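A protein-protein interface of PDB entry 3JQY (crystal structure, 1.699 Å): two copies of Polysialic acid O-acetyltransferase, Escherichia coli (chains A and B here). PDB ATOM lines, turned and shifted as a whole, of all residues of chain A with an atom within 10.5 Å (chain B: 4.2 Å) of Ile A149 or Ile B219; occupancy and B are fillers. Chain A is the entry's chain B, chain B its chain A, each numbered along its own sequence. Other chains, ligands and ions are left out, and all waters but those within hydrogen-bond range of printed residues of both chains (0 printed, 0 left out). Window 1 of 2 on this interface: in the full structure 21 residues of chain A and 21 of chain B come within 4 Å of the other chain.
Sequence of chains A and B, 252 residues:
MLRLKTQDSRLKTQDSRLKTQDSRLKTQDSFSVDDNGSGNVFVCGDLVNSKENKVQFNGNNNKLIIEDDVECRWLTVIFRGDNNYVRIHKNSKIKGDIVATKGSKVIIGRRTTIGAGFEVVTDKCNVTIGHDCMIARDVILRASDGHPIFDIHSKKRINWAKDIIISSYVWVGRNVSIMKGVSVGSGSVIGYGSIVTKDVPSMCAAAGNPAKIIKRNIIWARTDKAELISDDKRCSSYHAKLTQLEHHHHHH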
ATOM      1  N   ASP A 123       9.822 -37.493 -17.936  1.00  0.00           N
ATOM      2  CA  ASP A 123       8.634 -36.801 -17.454  1.00  0.00           C
ATOM      3  C   ASP A 123       7.426 -37.289 -18.253  1.00  0.00           C
ATOM      4  O   ASP A 123       7.237 -36.914 -19.410  1.00  0.00           O
ATOM      5  CB  ASP A 123       8.805 -35.282 -17.556  1.00  0.00           C
ATOM      6  CG  ASP A 123       7.547 -34.529 -17.184  1.00  0.00           C
ATOM      7  OD1 ASP A 123       6.659 -35.130 -16.545  1.00  0.00           O
ATOM      8  OD2 ASP A 123       7.445 -33.334 -17.534  1.00  0.00           O
ATOM      9  N   SER A 144      13.464 -35.468 -21.063  1.00  0.00           N
ATOM     10  CA  SER A 144      12.764 -34.281 -20.583  1.00  0.00           C
ATOM     11  C   SER A 144      13.747 -33.128 -20.391  1.00  0.00           C
ATOM     12  O   SER A 144      14.857 -33.336 -19.901  1.00  0.00           O
ATOM     13  CB  SER A 144      12.067 -34.583 -19.258  1.00  0.00           C
ATOM     14  OG  SER A 144      11.551 -33.395 -18.680  1.00  0.00           O
ATOM     15  N   ASP A 145      13.339 -31.912 -20.756  1.00  0.00           N
ATOM     16  CA  ASP A 145      14.222 -30.745 -20.656  1.00  0.00           C
ATOM     17  C   ASP A 145      14.380 -30.217 -19.236  1.00  0.00           C
ATOM     18  O   ASP A 145      15.342 -29.503 -18.940  1.00  0.00           O
ATOM     19  CB  ASP A 145      13.744 -29.600 -21.557  1.00  0.00           C
ATOM     20  CG  ASP A 145      14.007 -29.853 -23.024  1.00  0.00           C
ATOM     21  OD1 ASP A 145      14.601 -30.900 -23.362  1.00  0.00           O
ATOM     22  OD2 ASP A 145      13.612 -28.999 -23.847  1.00  0.00           O
ATOM     23  N   GLY A 146      13.431 -30.543 -18.368  1.00  0.00           N
ATOM     24  CA  GLY A 146      13.504 -30.128 -16.978  1.00  0.00           C
ATOM     25  C   GLY A 146      12.801 -28.813 -16.682  1.00  0.00           C
ATOM     26  O   GLY A 146      12.401 -28.560 -15.545  1.00  0.00           O
ATOM     27  N   HIS A 147      12.671 -27.964 -17.698  1.00  0.00           N
ATOM     28  CA  HIS A 147      11.955 -26.693 -17.560  1.00  0.00           C
ATOM     29  C   HIS A 147      11.221 -26.383 -18.854  1.00  0.00           C
ATOM     30  O   HIS A 147      11.673 -26.765 -19.933  1.00  0.00           O
ATOM     31  CB  HIS A 147      12.917 -25.545 -17.227  1.00  0.00           C
ATOM     32  CG  HIS A 147      13.717 -25.771 -15.983  1.00  0.00           C
ATOM     33  ND1 HIS A 147      13.274 -25.388 -14.736  1.00  0.00           N
ATOM     34  CD2 HIS A 147      14.930 -26.343 -15.795  1.00  0.00           C
ATOM     35  CE1 HIS A 147      14.182 -25.713 -13.832  1.00  0.00           C
ATOM     36  NE2 HIS A 147      15.195 -26.295 -14.449  1.00  0.00           N
ATOM     37  N   PRO A 148      10.083 -25.682 -18.753  1.00  0.00           N
ATOM     38  CA  PRO A 148       9.267 -25.476 -19.955  1.00  0.00           C
ATOM     39  C   PRO A 148       9.764 -24.339 -20.838  1.00  0.00           C
ATOM     40  O   PRO A 148      10.283 -23.337 -20.340  1.00  0.00           O
ATOM     41  CB  PRO A 148       7.890 -25.131 -19.388  1.00  0.00           C
ATOM     42  CG  PRO A 148       8.162 -24.549 -18.038  1.00  0.00           C
ATOM     43  CD  PRO A 148       9.435 -25.174 -17.531  1.00  0.00           C
ATOM     44  N   ILE A 149       9.597 -24.511 -22.146  1.00  0.00           N
ATOM     45  CA  ILE A 149       9.839 -23.452 -23.118  1.00  0.00           C
ATOM     46  C   ILE A 149       8.534 -23.232 -23.875  1.00  0.00           C
ATOM     47  O   ILE A 149       7.848 -24.197 -24.232  1.00  0.00           O
ATOM     48  CB  ILE A 149      10.965 -23.839 -24.093  1.00  0.00           C
ATOM     49  CG1 ILE A 149      12.285 -24.008 -23.329  1.00  0.00           C
ATOM     50  CG2 ILE A 149      11.101 -22.804 -25.214  1.00  0.00           C
ATOM     51  CD1 ILE A 149      13.433 -24.539 -24.173  1.00  0.00           C
ATOM     52  N   PHE A 150       8.195 -21.966 -24.109  1.00  0.00           N
ATOM     53  CA  PHE A 150       6.937 -21.599 -24.759  1.00  0.00           C
ATOM     54  C   PHE A 150       7.170 -20.840 -26.056  1.00  0.00           C
ATOM     55  O   PHE A 150       8.185 -20.154 -26.221  1.00  0.00           O
ATOM     56  CB  PHE A 150       6.098 -20.710 -23.834  1.00  0.00           C
ATOM     57  CG  PHE A 150       5.949 -21.249 -22.450  1.00  0.00           C
ATOM     58  CD1 PHE A 150       4.837 -22.001 -22.106  1.00  0.00           C
ATOM     59  CD2 PHE A 150       6.922 -21.015 -21.486  1.00  0.00           C
ATOM     60  CE1 PHE A 150       4.697 -22.514 -20.828  1.00  0.00           C
ATOM     61  CE2 PHE A 150       6.784 -21.530 -20.202  1.00  0.00           C
ATOM     62  CZ  PHE A 150       5.666 -22.273 -19.877  1.00  0.00           C
ATOM     63  N   ASP A 151       6.218 -20.952 -26.978  1.00  0.00           N
ATOM     64  CA  ASP A 151       6.189 -20.083 -28.148  1.00  0.00           C
ATOM     65  C   ASP A 151       5.601 -18.733 -27.732  1.00  0.00           C
ATOM     66  O   ASP A 151       4.576 -18.685 -27.048  1.00  0.00           O
ATOM     67  CB  ASP A 151       5.344 -20.722 -29.252  1.00  0.00           C
ATOM     68  CG  ASP A 151       5.223 -19.845 -30.477  1.00  0.00           C
ATOM     69  OD1 ASP A 151       6.006 -20.044 -31.427  1.00  0.00           O
ATOM     70  OD2 ASP A 151       4.352 -18.951 -30.486  1.00  0.00           O
ATOM     71  N   ILE A 152       6.248 -17.638 -28.126  1.00  0.00           N
ATOM     72  CA  ILE A 152       5.845 -16.317 -27.632  1.00  0.00           C
ATOM     73  C   ILE A 152       4.520 -15.842 -28.223  1.00  0.00           C
ATOM     74  O   ILE A 152       3.862 -14.956 -27.671  1.00  0.00           O
ATOM     75  CB  ILE A 152       6.925 -15.241 -27.876  1.00  0.00           C
ATOM     76  CG1 ILE A 152       7.237 -15.106 -29.366  1.00  0.00           C
ATOM     77  CG2 ILE A 152       8.192 -15.559 -27.084  1.00  0.00           C
ATOM     78  CD1 ILE A 152       8.262 -14.030 -29.666  1.00  0.00           C
ATOM     79  N   HIS A 153       4.134 -16.435 -29.344  1.00  0.00           N
ATOM     80  CA  HIS A 153       2.916 -16.026 -30.030  1.00  0.00           C
ATOM     81  C   HIS A 153       1.705 -16.837 -29.567  1.00  0.00           C
ATOM     82  O   HIS A 153       0.653 -16.275 -29.266  1.00  0.00           O
ATOM     83  CB  HIS A 153       3.108 -16.110 -31.544  1.00  0.00           C
ATOM     84  CG  HIS A 153       4.231 -15.258 -32.052  1.00  0.00           C
ATOM     85  ND1 HIS A 153       4.337 -13.915 -31.757  1.00  0.00           N
ATOM     86  CD2 HIS A 153       5.299 -15.556 -32.831  1.00  0.00           C
ATOM     87  CE1 HIS A 153       5.422 -13.423 -32.330  1.00  0.00           C
ATOM     88  NE2 HIS A 153       6.021 -14.398 -32.991  1.00  0.00           N
ATOM     89  N   SER A 154       1.862 -18.154 -29.492  1.00  0.00           N
ATOM     90  CA  SER A 154       0.781 -19.018 -29.020  1.00  0.00           C
ATOM     91  C   SER A 154       0.700 -19.041 -27.491  1.00  0.00           C
ATOM     92  O   SER A 154      -0.366 -19.283 -26.926  1.00  0.00           O
ATOM     93  CB  SER A 154       0.949 -20.440 -29.558  1.00  0.00           C
ATOM     94  OG  SER A 154       1.923 -21.154 -28.818  1.00  0.00           O
ATOM     95  N   LYS A 155       1.833 -18.793 -26.835  1.00  0.00           N
ATOM     96  CA  LYS A 155       1.916 -18.759 -25.374  1.00  0.00           C
ATOM     97  C   LYS A 155       1.898 -20.170 -24.779  1.00  0.00           C
ATOM     98  O   LYS A 155       1.908 -20.348 -23.560  1.00  0.00           O
ATOM     99  CB  LYS A 155       0.783 -17.915 -24.787  1.00  0.00           C
ATOM    100  CG  LYS A 155       0.496 -16.630 -25.558  1.00  0.00           C
ATOM    101  CD  LYS A 155       1.403 -15.490 -25.133  1.00  0.00           C
ATOM    102  CE  LYS A 155       0.867 -14.135 -25.617  1.00  0.00           C
ATOM    103  NZ  LYS A 155       1.163 -13.824 -27.058  1.00  0.00           N
ATOM    104  N   LYS A 156       1.883 -21.168 -25.655  1.00  0.00           N
ATOM    105  CA  LYS A 156       1.826 -22.563 -25.234  1.00  0.00           C
ATOM    106  C   LYS A 156       3.203 -23.210 -25.174  1.00  0.00           C
ATOM    107  O   LYS A 156       4.101 -22.864 -25.937  1.00  0.00           O
ATOM    108  CB  LYS A 156       0.939 -23.366 -26.181  1.00  0.00           C
ATOM    109  CG  LYS A 156      -0.536 -22.998 -26.109  1.00  0.00           C
ATOM    110  CD  LYS A 156      -1.356 -23.863 -27.051  1.00  0.00           C
ATOM    111  CE  LYS A 156      -0.836 -23.765 -28.476  1.00  0.00           C
ATOM    112  NZ  LYS A 156      -1.536 -24.709 -29.396  1.00  0.00           N
ATOM    113  N   ARG A 157       3.351 -24.163 -24.264  1.00  0.00           N
ATOM    114  CA  ARG A 157       4.589 -24.919 -24.146  1.00  0.00           C
ATOM    115  C   ARG A 157       4.871 -25.725 -25.415  1.00  0.00           C
ATOM    116  O   ARG A 157       3.959 -26.302 -26.012  1.00  0.00           O
ATOM    117  CB  ARG A 157       4.538 -25.832 -22.923  1.00  0.00           C
ATOM    118  CG  ARG A 157       5.729 -26.752 -22.825  1.00  0.00           C
ATOM    119  CD  ARG A 157       5.814 -27.457 -21.479  1.00  0.00           C
ATOM    120  NE  ARG A 157       7.079 -28.178 -21.400  1.00  0.00           N
ATOM    121  CZ  ARG A 157       7.426 -29.008 -20.425  1.00  0.00           C
ATOM    122  NH1 ARG A 157       6.599 -29.246 -19.418  1.00  0.00           N
ATOM    123  NH2 ARG A 157       8.608 -29.607 -20.465  1.00  0.00           N
ATOM    124  N   ILE A 158       6.135 -25.763 -25.827  1.00  0.00           N
ATOM    125  CA  ILE A 158       6.510 -26.458 -27.054  1.00  0.00           C
ATOM    126  C   ILE A 158       7.645 -27.462 -26.877  1.00  0.00           C
ATOM    127  O   ILE A 158       8.119 -28.041 -27.854  1.00  0.00           O
ATOM    128  CB  ILE A 158       6.880 -25.470 -28.173  1.00  0.00           C
ATOM    129  CG1 ILE A 158       8.027 -24.557 -27.718  1.00  0.00           C
ATOM    130  CG2 ILE A 158       5.651 -24.657 -28.568  1.00  0.00           C
ATOM    131  CD1 ILE A 158       8.589 -23.659 -28.816  1.00  0.00           C
ATOM    132  N   ASN A 159       8.093 -27.661 -25.641  1.00  0.00           N
ATOM    133  CA  ASN A 159       9.158 -28.628 -25.396  1.00  0.00           C
ATOM    134  C   ASN A 159       8.731 -29.773 -24.485  1.00  0.00           C
ATOM    135  O   ASN A 159       9.443 -30.129 -23.547  1.00  0.00           O
ATOM    136  CB  ASN A 159      10.410 -27.942 -24.840  1.00  0.00           C
ATOM    137  CG  ASN A 159      10.234 -27.467 -23.414  1.00  0.00           C
ATOM    138  OD1 ASN A 159       9.121 -27.167 -22.971  1.00  0.00           O
ATOM    139  ND2 ASN A 159      11.342 -27.379 -22.683  1.00  0.00           N
ATOM    140  N   TRP A 160       7.568 -30.349 -24.769  1.00  0.00           N
ATOM    141  CA  TRP A 160       7.087 -31.500 -24.015  1.00  0.00           C
ATOM    142  C   TRP A 160       8.075 -32.655 -24.149  1.00  0.00           C
ATOM    143  O   TRP A 160       8.710 -32.826 -25.195  1.00  0.00           O
ATOM    144  CB  TRP A 160       5.712 -31.942 -24.526  1.00  0.00           C
ATOM    145  CG  TRP A 160       4.627 -30.919 -24.327  1.00  0.00           C
ATOM    146  CD1 TRP A 160       4.082 -30.107 -25.280  1.00  0.00           C
ATOM    147  CD2 TRP A 160       3.959 -30.606 -23.100  1.00  0.00           C
ATOM    148  NE1 TRP A 160       3.113 -29.306 -24.720  1.00  0.00           N
ATOM    149  CE2 TRP A 160       3.018 -29.592 -23.384  1.00  0.00           C
ATOM    150  CE3 TRP A 160       4.065 -31.080 -21.788  1.00  0.00           C
ATOM    151  CZ2 TRP A 160       2.191 -29.045 -22.404  1.00  0.00           C
ATOM    152  CZ3 TRP A 160       3.240 -30.537 -20.816  1.00  0.00           C
ATOM    153  CH2 TRP A 160       2.315 -29.529 -21.130  1.00  0.00           C
ATOM    154  N   ALA A 161       8.204 -33.443 -23.086  1.00  0.00           N
ATOM    155  CA  ALA A 161       9.088 -34.606 -23.095  1.00  0.00           C
ATOM    156  C   ALA A 161       8.709 -35.576 -24.210  1.00  0.00           C
ATOM    157  O   ALA A 161       7.539 -35.689 -24.586  1.00  0.00           O
ATOM    158  CB  ALA A 161       9.054 -35.302 -21.734  1.00  0.00           C
ATOM    159  N   LYS A 180      15.764 -35.673 -26.299  1.00  0.00           N
ATOM    160  CA  LYS A 180      14.393 -36.170 -26.334  1.00  0.00           C
ATOM    161  C   LYS A 180      13.885 -36.506 -27.737  1.00  0.00           C
ATOM    162  O   LYS A 180      14.242 -35.861 -28.722  1.00  0.00           O
ATOM    163  CB  LYS A 180      13.446 -35.185 -25.640  1.00  0.00           C
ATOM    164  CG  LYS A 180      13.265 -33.867 -26.381  1.00  0.00           C
ATOM    165  CD  LYS A 180      12.262 -32.970 -25.651  1.00  0.00           C
ATOM    166  CE  LYS A 180      12.165 -31.601 -26.300  1.00  0.00           C
ATOM    167  NZ  LYS A 180      13.477 -30.891 -26.297  1.00  0.00           N
ATOM    168  N   TYR B 169      16.955 -12.609 -17.444  1.00  0.00           N
ATOM    169  CA  TYR B 169      16.014 -13.680 -17.759  1.00  0.00           C
ATOM    170  C   TYR B 169      16.520 -14.592 -18.883  1.00  0.00           C
ATOM    171  O   TYR B 169      15.820 -14.856 -19.863  1.00  0.00           O
ATOM    172  CB  TYR B 169      14.609 -13.129 -18.059  1.00  0.00           C
ATOM    173  CG  TYR B 169      13.532 -14.164 -17.820  1.00  0.00           C
ATOM    174  CD1 TYR B 169      13.324 -14.676 -16.552  1.00  0.00           C
ATOM    175  CD2 TYR B 169      12.752 -14.650 -18.865  1.00  0.00           C
ATOM    176  CE1 TYR B 169      12.360 -15.640 -16.308  1.00  0.00           C
ATOM    177  CE2 TYR B 169      11.763 -15.622 -18.630  1.00  0.00           C
ATOM    178  CZ  TYR B 169      11.581 -16.108 -17.347  1.00  0.00           C
ATOM    179  OH  TYR B 169      10.626 -17.068 -17.085  1.00  0.00           O
ATOM    180  N   TRP B 171      18.243 -18.488 -19.544  1.00  0.00           N
ATOM    181  CA  TRP B 171      18.496 -19.822 -19.016  1.00  0.00           C
ATOM    182  C   TRP B 171      19.725 -20.380 -19.724  1.00  0.00           C
ATOM    183  O   TRP B 171      19.691 -20.627 -20.938  1.00  0.00           O
ATOM    184  CB  TRP B 171      17.273 -20.716 -19.241  1.00  0.00           C
ATOM    185  CG  TRP B 171      17.481 -22.192 -18.947  1.00  0.00           C
ATOM    186  CD1 TRP B 171      18.498 -22.758 -18.240  1.00  0.00           C
ATOM    187  CD2 TRP B 171      16.617 -23.269 -19.340  1.00  0.00           C
ATOM    188  NE1 TRP B 171      18.333 -24.128 -18.175  1.00  0.00           N
ATOM    189  CE2 TRP B 171      17.181 -24.463 -18.840  1.00  0.00           C
ATOM    190  CE3 TRP B 171      15.427 -23.337 -20.069  1.00  0.00           C
ATOM    191  CZ2 TRP B 171      16.599 -25.712 -19.059  1.00  0.00           C
ATOM    192  CZ3 TRP B 171      14.843 -24.578 -20.275  1.00  0.00           C
ATOM    193  CH2 TRP B 171      15.431 -25.748 -19.775  1.00  0.00           C
ATOM    194  N   GLY B 187      15.376 -13.567 -22.316  1.00  0.00           N
ATOM    195  CA  GLY B 187      14.391 -14.599 -22.593  1.00  0.00           C
ATOM    196  C   GLY B 187      14.928 -15.813 -23.322  1.00  0.00           C
ATOM    197  O   GLY B 187      14.200 -16.776 -23.574  1.00  0.00           O
ATOM    198  N   ILE B 218      10.835 -17.797 -28.791  1.00  0.00           N
ATOM    199  CA  ILE B 218      10.564 -18.585 -27.592  1.00  0.00           C
ATOM    200  C   ILE B 218      10.906 -17.838 -26.308  1.00  0.00           C
ATOM    201  O   ILE B 218      11.591 -16.814 -26.329  1.00  0.00           O
ATOM    202  CB  ILE B 218      11.333 -19.934 -27.604  1.00  0.00           C
ATOM    203  CG1 ILE B 218      12.847 -19.701 -27.652  1.00  0.00           C
ATOM    204  CG2 ILE B 218      10.905 -20.777 -28.783  1.00  0.00           C
ATOM    205  CD1 ILE B 218      13.501 -19.567 -26.296  1.00  0.00           C
ATOM    206  N   ILE B 219      10.417 -18.374 -25.195  1.00  0.00           N
ATOM    207  CA  ILE B 219      10.744 -17.886 -23.862  1.00  0.00           C
ATOM    208  C   ILE B 219      10.582 -19.068 -22.903  1.00  0.00           C
ATOM    209  O   ILE B 219       9.815 -19.989 -23.181  1.00  0.00           O
ATOM    210  CB  ILE B 219       9.838 -16.707 -23.446  1.00  0.00           C
ATOM    211  CG1 ILE B 219      10.460 -15.933 -22.280  1.00  0.00           C
ATOM    212  CG2 ILE B 219       8.425 -17.188 -23.098  1.00  0.00           C
ATOM    213  CD1 ILE B 219       9.798 -14.587 -22.012  1.00  0.00           C
ATOM    214  N   TRP B 220      11.311 -19.047 -21.791  1.00  0.00           N
ATOM    215  CA  TRP B 220      11.325 -20.167 -20.843  1.00  0.00           C
ATOM    216  C   TRP B 220      10.721 -19.758 -19.506  1.00  0.00           C
ATOM    217  O   TRP B 220      10.518 -18.574 -19.247  1.00  0.00           O
ATOM    218  CB  TRP B 220      12.769 -20.627 -20.614  1.00  0.00           C
ATOM    219  CG  TRP B 220      13.602 -19.528 -20.016  1.00  0.00           C
ATOM    220  CD1 TRP B 220      14.165 -18.475 -20.678  1.00  0.00           C
ATOM    221  CD2 TRP B 220      13.921 -19.348 -18.628  1.00  0.00           C
ATOM    222  NE1 TRP B 220      14.828 -17.656 -19.793  1.00  0.00           N
ATOM    223  CE2 TRP B 220      14.693 -18.168 -18.527  1.00  0.00           C
ATOM    224  CE3 TRP B 220      13.644 -20.078 -17.465  1.00  0.00           C
ATOM    225  CZ2 TRP B 220      15.193 -17.702 -17.308  1.00  0.00           C
ATOM    226  CZ3 TRP B 220      14.137 -19.605 -16.247  1.00  0.00           C
ATOM    227  CH2 TRP B 220      14.898 -18.431 -16.181  1.00  0.00           C
ATOM    228  N   ILE B 229       2.386 -19.502 -20.773  1.00  0.00           N
ATOM    229  CA  ILE B 229       3.186 -18.399 -20.259  1.00  0.00           C
ATOM    230  C   ILE B 229       2.537 -17.763 -19.025  1.00  0.00           C
ATOM    231  O   ILE B 229       3.223 -17.423 -18.058  1.00  0.00           O
ATOM    232  CB  ILE B 229       3.429 -17.335 -21.343  1.00  0.00           C
ATOM    233  CG1 ILE B 229       4.426 -17.868 -22.379  1.00  0.00           C
ATOM    234  CG2 ILE B 229       3.927 -16.042 -20.718  1.00  0.00           C
ATOM    235  CD1 ILE B 229       4.710 -16.918 -23.517  1.00  0.00           C
ATOM    236  N   CYS B 235       7.842 -15.242 -16.003  1.00  0.00           N
ATOM    237  CA  CYS B 235       7.747 -15.471 -17.437  1.00  0.00           C
ATOM    238  C   CYS B 235       6.766 -14.484 -18.066  1.00  0.00           C
ATOM    239  O   CYS B 235       7.071 -13.844 -19.072  1.00  0.00           O
ATOM    240  CB  CYS B 235       7.292 -16.907 -17.710  1.00  0.00           C
ATOM    241  SG  CYS B 235       7.301 -17.358 -19.447  1.00  0.00           S
ATOM    242  N   HIS B 239       7.725 -11.671 -20.702  1.00  0.00           N
ATOM    243  CA  HIS B 239       7.020 -11.809 -21.969  1.00  0.00           C
ATOM    244  C   HIS B 239       6.359 -10.490 -22.365  1.00  0.00           C
ATOM    245  O   HIS B 239       6.482 -10.043 -23.502  1.00  0.00           O
ATOM    246  CB  HIS B 239       5.976 -12.926 -21.885  1.00  0.00           C
ATOM    247  CG  HIS B 239       5.150 -13.077 -23.125  1.00  0.00           C
ATOM    248  ND1 HIS B 239       5.613 -13.707 -24.261  1.00  0.00           N
ATOM    249  CD2 HIS B 239       3.888 -12.673 -23.405  1.00  0.00           C
ATOM    250  CE1 HIS B 239       4.671 -13.685 -25.188  1.00  0.00           C
ATOM    251  NE2 HIS B 239       3.616 -13.064 -24.695  1.00  0.00           N
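N of Phe A150 lies within hydrogen-bond range of O of Ile B219, at 2.7 Å. The side-chain amino group (NZ) of Lys A155 sits close to a ring nitrogen (NE2) of His B239, at 3.5 Å. The backbone carbonyl oxygen (O) of Lys A155 is in hydrogen-bond range of the backbone NH (N) of Ile B229.
The backbone carbonyl oxygen of His A147 is in hydrogen-bond range of the side-chain amide nitrogen of Asn A159 (2.8 Å). O of His A153 lies within hydrogen-bond range of NZ of Lys A155. The backbone NH of Ile A149 sits at hydrogen-bond distance from the side-chain amide oxygen of Asn A159. The side-chain carboxylate (OD2) of Asp A151 sits at hydrogen-bond distance from the backbone NH (N) of His A153. SG of Cys B235 is in hydrogen-bond range of O of Trp B220. OD2 of Asp A151 lies within hydrogen-bond range of N of Ser A154, at 2.8 Å.
Asp A145 touches Trp B171 (O to CH2, 3.8 Å). CH2 of Trp B171 touches CB of His A147, at 3.6 Å. Trp B220 touches Pro A148 (CA to O, 3.4 Å). Ile A149 touches Ile B218 (CG2 to CB, 3.7 Å). Ile A149 touches Ile B219 (CA to O, 3.5 Å). Phe A150 touches Ile B218. CB of Phe A150 touches CG1 of Ile B229, 3.6 Å away. Asp A151 touches Ile B229 (O to CD1, 3.95 Å). Ile A152 touches His B239 (O to CE1, 2.9 Å). CG2 of Ile B218 touches CD1 of Ile A158, at 3.7 Å.
Of chain B, only Ile B218 (3.7 Å) and Ile B219 (3.5 Å) come within 4 Å of Ile A149. Ile B219 touches just these residues of chain A: Ile A149 and Phe A150. Ile B218 touches just these residues of chain A: Ile A149, Phe A150, Ile A152 and Ile A158. No residue of chain A comes within 4 Å of Cys B235. Printed residues of chain B within 4 Å of Ile A152: Ile B218 and His B239. Of the printed residues of chain A, His B239 touches Ile A152 (2.9 Å) and Lys A155 (3.1 Å). The nearest residue of chain A that does not touch Ile B219 is Ile A152 (4.1 Å).
Of the 9 printed residues of chain B, 6 touch a printed residue of chain A. Hydrophobic or aromatic side chains of chain B within 4 Å of the printed part of chain A: Trp B171, Ile B218, Trp B220, Ile B229 and His B239. Printed residues of chain A that touch a printed residue of chain B: Asp A145, His A147, Pro A148, Ile A149, Phe A150, Asp A151, Ile A152, Lys A155 and Ile A158. Along chain A the printed residues that touch a printed residue of chain B span positions 145 to 158. Among the printed residues, 14 pairs touch across the chains.
No position is printed for both chains. Of the 14 pairs that touch across the chains among the printed residues, none has its exchanged pair printed and touching as well.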
